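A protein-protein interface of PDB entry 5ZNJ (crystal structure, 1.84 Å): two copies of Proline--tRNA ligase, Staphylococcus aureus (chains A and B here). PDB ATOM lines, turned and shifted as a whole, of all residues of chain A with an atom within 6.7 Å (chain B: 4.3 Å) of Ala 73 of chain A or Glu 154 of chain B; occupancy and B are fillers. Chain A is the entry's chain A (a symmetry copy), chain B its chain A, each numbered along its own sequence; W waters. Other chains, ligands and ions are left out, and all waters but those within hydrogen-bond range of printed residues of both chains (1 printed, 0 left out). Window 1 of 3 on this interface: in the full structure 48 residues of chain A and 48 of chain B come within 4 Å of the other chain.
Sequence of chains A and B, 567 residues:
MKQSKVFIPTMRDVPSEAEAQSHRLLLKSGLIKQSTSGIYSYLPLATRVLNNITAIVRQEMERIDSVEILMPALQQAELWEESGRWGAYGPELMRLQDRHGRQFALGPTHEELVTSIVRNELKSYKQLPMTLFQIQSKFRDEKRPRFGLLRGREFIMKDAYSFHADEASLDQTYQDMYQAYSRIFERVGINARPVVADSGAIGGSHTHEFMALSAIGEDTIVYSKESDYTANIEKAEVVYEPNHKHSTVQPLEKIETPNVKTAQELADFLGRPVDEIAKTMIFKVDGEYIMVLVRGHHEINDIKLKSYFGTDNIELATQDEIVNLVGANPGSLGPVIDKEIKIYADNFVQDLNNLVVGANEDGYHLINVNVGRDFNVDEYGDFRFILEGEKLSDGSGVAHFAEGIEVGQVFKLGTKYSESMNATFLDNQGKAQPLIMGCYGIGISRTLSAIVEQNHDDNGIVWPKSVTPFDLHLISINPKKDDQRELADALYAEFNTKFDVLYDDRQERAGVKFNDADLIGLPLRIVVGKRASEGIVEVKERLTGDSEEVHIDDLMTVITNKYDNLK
The side-chain carboxylate (OE1) of Glu 154 of chain B sits at hydrogen-bond distance from the backbone NH (N) of Leu 74 of chain A, 2.9 Å away. The side-chain carboxylate (OE2) of Glu 154 of chain B sits at hydrogen-bond distance from the backbone NH (N) of Ala 73 of chain A (3.0 Å).
O of Ala 73 of chain A sits at hydrogen-bond distance from N of Gly 107 of chain A (2.8 Å). A ring nitrogen (NE2) of His 110 of chain A sits at hydrogen-bond distance from the backbone carbonyl oxygen (O) of Pro 72 of chain A (2.9 Å). NE2 of Gln 75 of chain A is in hydrogen-bond range of O of Pro 72 of chain A (3.2 Å).
CA of Pro 72 of chain A touches OE2 of Glu 154 of chain B (3.5 Å). Leu 74 of chain A touches Phe 139 of chain B (CD1 to CD2, 3.6 Å).
Of chain B, only Glu 154 comes within 4 Å of Ala 73 of chain A. Printed residues of chain A within 4 Å of Glu 154 of chain B: Pro 72 (3.5 Å), Ala 73 (3.0 Å) and Leu 74 (2.9 Å). Printed residues of chain A within 4 Å of Phe 139 of chain B: Leu 74 (3.6 Å). Of the printed residues of chain B, Leu 74 of chain A touches Phe 139 (3.6 Å) and Glu 154 (2.9 Å). The nearest residue of chain B that does not touch Ala 73 of chain A is Phe 139 of chain B (4.03 Å). The nearest printed residue of chain A that does not touch Glu 154 of chain B is Met 71 of chain A (4.7 Å).
Printed residues of chain B that touch a printed residue of chain A: Phe 139 and Glu 154. Printed residues of chain A that touch a printed residue of chain B: Pro 72, Ala 73 and Leu 74. Hydrophobic or aromatic side chains of chain A that line the printed part of chain B: Pro 72, Ala 73 and Leu 74. Among the printed residues, 4 pairs touch across the chains.
Position printed for both chains: 139.
Water W1 lies within hydrogen-bond range of the backbone carbonyl oxygen of Met 71 of chain A (2.9 Å), the side-chain carboxylate of Glu 154 of chain B (3.0 Å) and the side-chain amide nitrogen of Gln 136 of chain A (3.1 Å).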
ATOM      1  N   MET A  71     -22.870 -27.347 -19.147  1.00  0.00           N
ATOM      2  CA  MET A  71     -23.241 -26.008 -18.748  1.00  0.00           C
ATOM      3  C   MET A  71     -23.468 -25.970 -17.241  1.00  0.00           C
ATOM      4  O   MET A  71     -23.695 -27.019 -16.614  1.00  0.00           O
ATOM      5  CB  MET A  71     -24.502 -25.561 -19.483  1.00  0.00           C
ATOM      6  CG  MET A  71     -24.325 -25.437 -20.982  1.00  0.00           C
ATOM      7  SD  MET A  71     -25.824 -24.884 -21.801  1.00  0.00           S
ATOM      8  CE  MET A  71     -26.728 -26.429 -21.932  1.00  0.00           C
ATOM      9  N   PRO A  72     -23.390 -24.768 -16.651  1.00  0.00           N
ATOM     10  CA  PRO A  72     -23.488 -24.631 -15.196  1.00  0.00           C
ATOM     11  C   PRO A  72     -24.913 -24.745 -14.646  1.00  0.00           C
ATOM     12  O   PRO A  72     -25.894 -24.450 -15.344  1.00  0.00           O
ATOM     13  CB  PRO A  72     -22.917 -23.227 -14.941  1.00  0.00           C
ATOM     14  CG  PRO A  72     -23.143 -22.493 -16.212  1.00  0.00           C
ATOM     15  CD  PRO A  72     -22.940 -23.509 -17.282  1.00  0.00           C
ATOM     16  N   ALA A  73     -25.012 -25.198 -13.401  1.00  0.00           N
ATOM     17  CA  ALA A  73     -26.266 -25.162 -12.636  1.00  0.00           C
ATOM     18  C   ALA A  73     -26.574 -23.745 -12.134  1.00  0.00           C
ATOM     19  O   ALA A  73     -27.729 -23.306 -12.171  1.00  0.00           O
ATOM     20  CB  ALA A  73     -26.179 -26.118 -11.454  1.00  0.00           C
ATOM     21  N   LEU A  74     -25.538 -23.041 -11.671  1.00  0.00           N
ATOM     22  CA  LEU A  74     -25.690 -21.686 -11.110  1.00  0.00           C
ATOM     23  C   LEU A  74     -25.824 -20.670 -12.229  1.00  0.00           C
ATOM     24  O   LEU A  74     -24.873 -20.443 -12.978  1.00  0.00           O
ATOM     25  CB  LEU A  74     -24.487 -21.297 -10.247  1.00  0.00           C
ATOM     26  CG  LEU A  74     -24.503 -21.639  -8.768  1.00  0.00           C
ATOM     27  CD1 LEU A  74     -23.177 -21.204  -8.166  1.00  0.00           C
ATOM     28  CD2 LEU A  74     -25.665 -20.965  -8.056  1.00  0.00           C
ATOM     29  N   GLN A  75     -26.993 -20.044 -12.347  1.00  0.00           N
ATOM     30  CA  GLN A  75     -27.269 -19.150 -13.473  1.00  0.00           C
ATOM     31  C   GLN A  75     -27.777 -17.797 -13.001  1.00  0.00           C
ATOM     32  O   GLN A  75     -28.726 -17.720 -12.212  1.00  0.00           O
ATOM     33  CB  GLN A  75     -28.278 -19.789 -14.416  1.00  0.00           C
ATOM     34  CG  GLN A  75     -27.850 -21.164 -14.924  1.00  0.00           C
ATOM     35  CD  GLN A  75     -28.850 -21.805 -15.867  1.00  0.00           C
ATOM     36  OE1 GLN A  75     -29.780 -21.160 -16.361  1.00  0.00           O
ATOM     37  NE2 GLN A  75     -28.656 -23.083 -16.130  1.00  0.00           N
ATOM     38  N   TRP A  80     -32.220 -14.996 -16.871  1.00  0.00           N
ATOM     39  CA  TRP A  80     -33.617 -15.412 -16.769  1.00  0.00           C
ATOM     40  C   TRP A  80     -34.592 -14.234 -16.917  1.00  0.00           C
ATOM     41  O   TRP A  80     -35.739 -14.424 -17.325  1.00  0.00           O
ATOM     42  CB  TRP A  80     -33.830 -16.187 -15.464  1.00  0.00           C
ATOM     43  CG  TRP A  80     -33.180 -17.542 -15.549  1.00  0.00           C
ATOM     44  CD1 TRP A  80     -31.855 -17.836 -15.407  1.00  0.00           C
ATOM     45  CD2 TRP A  80     -33.830 -18.768 -15.883  1.00  0.00           C
ATOM     46  NE1 TRP A  80     -31.645 -19.187 -15.608  1.00  0.00           N
ATOM     47  CE2 TRP A  80     -32.846 -19.780 -15.895  1.00  0.00           C
ATOM     48  CE3 TRP A  80     -35.161 -19.115 -16.147  1.00  0.00           C
ATOM     49  CZ2 TRP A  80     -33.152 -21.119 -16.171  1.00  0.00           C
ATOM     50  CZ3 TRP A  80     -35.465 -20.443 -16.418  1.00  0.00           C
ATOM     51  CH2 TRP A  80     -34.462 -21.427 -16.437  1.00  0.00           C
ATOM     52  N   ALA A 105     -30.568 -18.380 -10.329  1.00  0.00           N
ATOM     53  CA  ALA A 105     -31.395 -19.578 -10.385  1.00  0.00           C
ATOM     54  C   ALA A 105     -30.489 -20.799 -10.435  1.00  0.00           C
ATOM     55  O   ALA A 105     -29.377 -20.735 -10.976  1.00  0.00           O
ATOM     56  CB  ALA A 105     -32.275 -19.561 -11.617  1.00  0.00           C
ATOM     57  N   LEU A 106     -30.966 -21.901  -9.871  1.00  0.00           N
ATOM     58  CA  LEU A 106     -30.394 -23.214 -10.172  1.00  0.00           C
ATOM     59  C   LEU A 106     -31.136 -23.739 -11.393  1.00  0.00           C
ATOM     60  O   LEU A 106     -32.363 -23.739 -11.413  1.00  0.00           O
ATOM     61  CB  LEU A 106     -30.525 -24.169  -8.992  1.00  0.00           C
ATOM     62  CG  LEU A 106     -29.743 -23.804  -7.728  1.00  0.00           C
ATOM     63  CD1 LEU A 106     -30.117 -24.754  -6.599  1.00  0.00           C
ATOM     64  CD2 LEU A 106     -28.242 -23.828  -7.979  1.00  0.00           C
ATOM     65  N   GLY A 107     -30.398 -24.158 -12.418  1.00  0.00           N
ATOM     66  CA  GLY A 107     -30.997 -24.533 -13.699  1.00  0.00           C
ATOM     67  C   GLY A 107     -32.029 -25.663 -13.619  1.00  0.00           C
ATOM     68  O   GLY A 107     -31.688 -26.760 -13.200  1.00  0.00           O
ATOM     69  N   PRO A 108     -33.296 -25.396 -14.008  1.00  0.00           N
ATOM     70  CA  PRO A 108     -34.276 -26.483 -14.221  1.00  0.00           C
ATOM     71  C   PRO A 108     -34.239 -27.059 -15.635  1.00  0.00           C
ATOM     72  O   PRO A 108     -34.857 -28.093 -15.900  1.00  0.00           O
ATOM     73  CB  PRO A 108     -35.610 -25.782 -13.990  1.00  0.00           C
ATOM     74  CG  PRO A 108     -35.376 -24.387 -14.444  1.00  0.00           C
ATOM     75  CD  PRO A 108     -33.936 -24.068 -14.154  1.00  0.00           C
ATOM     76  N   HIS A 110     -32.075 -25.386 -19.652  1.00  0.00           N
ATOM     77  CA  HIS A 110     -30.939 -24.520 -20.038  1.00  0.00           C
ATOM     78  C   HIS A 110     -31.123 -23.698 -21.329  1.00  0.00           C
ATOM     79  O   HIS A 110     -30.133 -23.324 -21.969  1.00  0.00           O
ATOM     80  CB  HIS A 110     -29.656 -25.375 -20.102  1.00  0.00           C
ATOM     81  CG  HIS A 110     -29.070 -25.695 -18.763  1.00  0.00           C
ATOM     82  ND1 HIS A 110     -29.703 -26.501 -17.842  1.00  0.00           N
ATOM     83  CD2 HIS A 110     -27.895 -25.334 -18.197  1.00  0.00           C
ATOM     84  CE1 HIS A 110     -28.955 -26.608 -16.759  1.00  0.00           C
ATOM     85  NE2 HIS A 110     -27.845 -25.917 -16.953  1.00  0.00           N
ATOM     86  N   GLN A 136     -26.568 -33.585 -17.242  1.00  0.00           N
ATOM     87  CA  GLN A 136     -26.334 -32.650 -16.162  1.00  0.00           C
ATOM     88  C   GLN A 136     -27.526 -32.619 -15.222  1.00  0.00           C
ATOM     89  O   GLN A 136     -28.683 -32.805 -15.647  1.00  0.00           O
ATOM     90  CB  GLN A 136     -26.022 -31.280 -16.784  1.00  0.00           C
ATOM     91  CG  GLN A 136     -25.570 -30.192 -15.831  1.00  0.00           C
ATOM     92  CD  GLN A 136     -26.688 -29.261 -15.385  1.00  0.00           C
ATOM     93  OE1 GLN A 136     -27.865 -29.460 -15.706  1.00  0.00           O
ATOM     94  NE2 GLN A 136     -26.325 -28.249 -14.621  1.00  0.00           N
ATOM     95  N   SER A 137     -27.243 -32.435 -13.935  1.00  0.00           N
ATOM     96  CA  SER A 137     -28.294 -32.471 -12.923  1.00  0.00           C
ATOM     97  C   SER A 137     -29.072 -31.163 -12.892  1.00  0.00           C
ATOM     98  O   SER A 137     -28.486 -30.085 -12.779  1.00  0.00           O
ATOM     99  CB  SER A 137     -27.738 -32.831 -11.548  1.00  0.00           C
ATOM    100  OG  SER A 137     -27.440 -34.220 -11.517  1.00  0.00           O
ATOM    101  N   PHE A 139     -32.479 -28.874 -11.303  1.00  0.00           N
ATOM    102  CA  PHE A 139     -33.120 -28.557 -10.027  1.00  0.00           C
ATOM    103  C   PHE A 139     -34.511 -28.009 -10.284  1.00  0.00           C
ATOM    104  O   PHE A 139     -34.667 -27.048 -11.044  1.00  0.00           O
ATOM    105  CB  PHE A 139     -32.286 -27.526  -9.262  1.00  0.00           C
ATOM    106  CG  PHE A 139     -30.896 -28.001  -8.957  1.00  0.00           C
ATOM    107  CD1 PHE A 139     -29.873 -27.825  -9.877  1.00  0.00           C
ATOM    108  CD2 PHE A 139     -30.617 -28.660  -7.764  1.00  0.00           C
ATOM    109  CE1 PHE A 139     -28.595 -28.285  -9.608  1.00  0.00           C
ATOM    110  CE2 PHE A 139     -29.334 -29.115  -7.485  1.00  0.00           C
ATOM    111  CZ  PHE A 139     -28.325 -28.941  -8.412  1.00  0.00           C
ATOM    112  N   GLY B  38     -16.359 -16.715 -12.120  1.00  0.00           N
ATOM    113  CA  GLY B  38     -16.106 -18.049 -11.594  1.00  0.00           C
ATOM    114  C   GLY B  38     -17.020 -19.153 -12.088  1.00  0.00           C
ATOM    115  O   GLY B  38     -16.973 -20.262 -11.546  1.00  0.00           O
ATOM    116  N   LYS B 138     -18.934 -29.066  -7.401  1.00  0.00           N
ATOM    117  CA  LYS B 138     -18.977 -28.431  -6.090  1.00  0.00           C
ATOM    118  C   LYS B 138     -19.245 -26.943  -6.239  1.00  0.00           C
ATOM    119  O   LYS B 138     -18.985 -26.359  -7.296  1.00  0.00           O
ATOM    120  CB  LYS B 138     -17.641 -28.609  -5.383  1.00  0.00           C
ATOM    121  CG  LYS B 138     -17.171 -30.047  -5.261  1.00  0.00           C
ATOM    122  CD  LYS B 138     -18.070 -30.880  -4.363  1.00  0.00           C
ATOM    123  CE  LYS B 138     -17.557 -32.309  -4.276  1.00  0.00           C
ATOM    124  NZ  LYS B 138     -17.811 -33.050  -5.528  1.00  0.00           N
ATOM    125  N   PHE B 139     -19.767 -26.348  -5.167  1.00  0.00           N
ATOM    126  CA  PHE B 139     -20.113 -24.927  -5.114  1.00  0.00           C
ATOM    127  C   PHE B 139     -19.401 -24.279  -3.941  1.00  0.00           C
ATOM    128  O   PHE B 139     -19.524 -24.750  -2.806  1.00  0.00           O
ATOM    129  CB  PHE B 139     -21.627 -24.761  -4.962  1.00  0.00           C
ATOM    130  CG  PHE B 139     -22.403 -25.367  -6.095  1.00  0.00           C
ATOM    131  CD1 PHE B 139     -22.766 -26.705  -6.064  1.00  0.00           C
ATOM    132  CD2 PHE B 139     -22.739 -24.609  -7.211  1.00  0.00           C
ATOM    133  CE1 PHE B 139     -23.460 -27.273  -7.118  1.00  0.00           C
ATOM    134  CE2 PHE B 139     -23.445 -25.170  -8.268  1.00  0.00           C
ATOM    135  CZ  PHE B 139     -23.793 -26.506  -8.230  1.00  0.00           C
ATOM    136  N   GLY B 152     -12.766 -21.450  -9.711  1.00  0.00           N
ATOM    137  CA  GLY B 152     -14.166 -21.192  -9.997  1.00  0.00           C
ATOM    138  C   GLY B 152     -15.043 -21.201  -8.755  1.00  0.00           C
ATOM    139  O   GLY B 152     -14.608 -21.551  -7.654  1.00  0.00           O
ATOM    140  N   ARG B 153     -16.298 -20.810  -8.952  1.00  0.00           N
ATOM    141  CA  ARG B 153     -17.323 -20.916  -7.923  1.00  0.00           C
ATOM    142  C   ARG B 153     -18.156 -22.179  -8.079  1.00  0.00           C
ATOM    143  O   ARG B 153     -18.641 -22.718  -7.093  1.00  0.00           O
ATOM    144  CB  ARG B 153     -18.211 -19.677  -7.934  1.00  0.00           C
ATOM    145  CG  ARG B 153     -17.443 -18.436  -7.518  1.00  0.00           C
ATOM    146  CD  ARG B 153     -18.377 -17.322  -7.101  1.00  0.00           C
ATOM    147  NE  ARG B 153     -19.007 -16.676  -8.249  1.00  0.00           N
ATOM    148  CZ  ARG B 153     -20.050 -15.849  -8.183  1.00  0.00           C
ATOM    149  NH1 ARG B 153     -20.640 -15.576  -7.017  1.00  0.00           N
ATOM    150  NH2 ARG B 153     -20.523 -15.303  -9.298  1.00  0.00           N
ATOM    151  N   GLU B 154     -18.325 -22.635  -9.317  1.00  0.00           N
ATOM    152  CA  GLU B 154     -18.869 -23.961  -9.600  1.00  0.00           C
ATOM    153  C   GLU B 154     -17.754 -24.708 -10.324  1.00  0.00           C
ATOM    154  O   GLU B 154     -17.275 -24.243 -11.347  1.00  0.00           O
ATOM    155  CB  GLU B 154     -20.133 -23.859 -10.463  1.00  0.00           C
ATOM    156  CG  GLU B 154     -20.800 -25.207 -10.753  1.00  0.00           C
ATOM    157  CD  GLU B 154     -22.111 -25.099 -11.507  1.00  0.00           C
ATOM    158  OE1 GLU B 154     -22.779 -24.036 -11.452  1.00  0.00           O
ATOM    159  OE2 GLU B 154     -22.478 -26.094 -12.175  1.00  0.00           O
ATOM    160  N   PHE B 155     -17.304 -25.831  -9.770  1.00  0.00           N
ATOM    161  CA  PHE B 155     -16.152 -26.543 -10.324  1.00  0.00           C
ATOM    162  C   PHE B 155     -16.296 -28.041 -10.120  1.00  0.00           C
ATOM    163  O   PHE B 155     -16.989 -28.478  -9.204  1.00  0.00           O
ATOM    164  CB  PHE B 155     -14.836 -26.038  -9.701  1.00  0.00           C
ATOM    165  CG  PHE B 155     -14.719 -26.279  -8.218  1.00  0.00           C
ATOM    166  CD1 PHE B 155     -15.257 -25.373  -7.311  1.00  0.00           C
ATOM    167  CD2 PHE B 155     -14.048 -27.396  -7.730  1.00  0.00           C
ATOM    168  CE1 PHE B 155     -15.148 -25.587  -5.944  1.00  0.00           C
ATOM    169  CE2 PHE B 155     -13.932 -27.616  -6.366  1.00  0.00           C
ATOM    170  CZ  PHE B 155     -14.479 -26.703  -5.467  1.00  0.00           C
HETATM  171  O   HOH W   1     -23.286 -28.258 -14.027  1.00  0.00           O
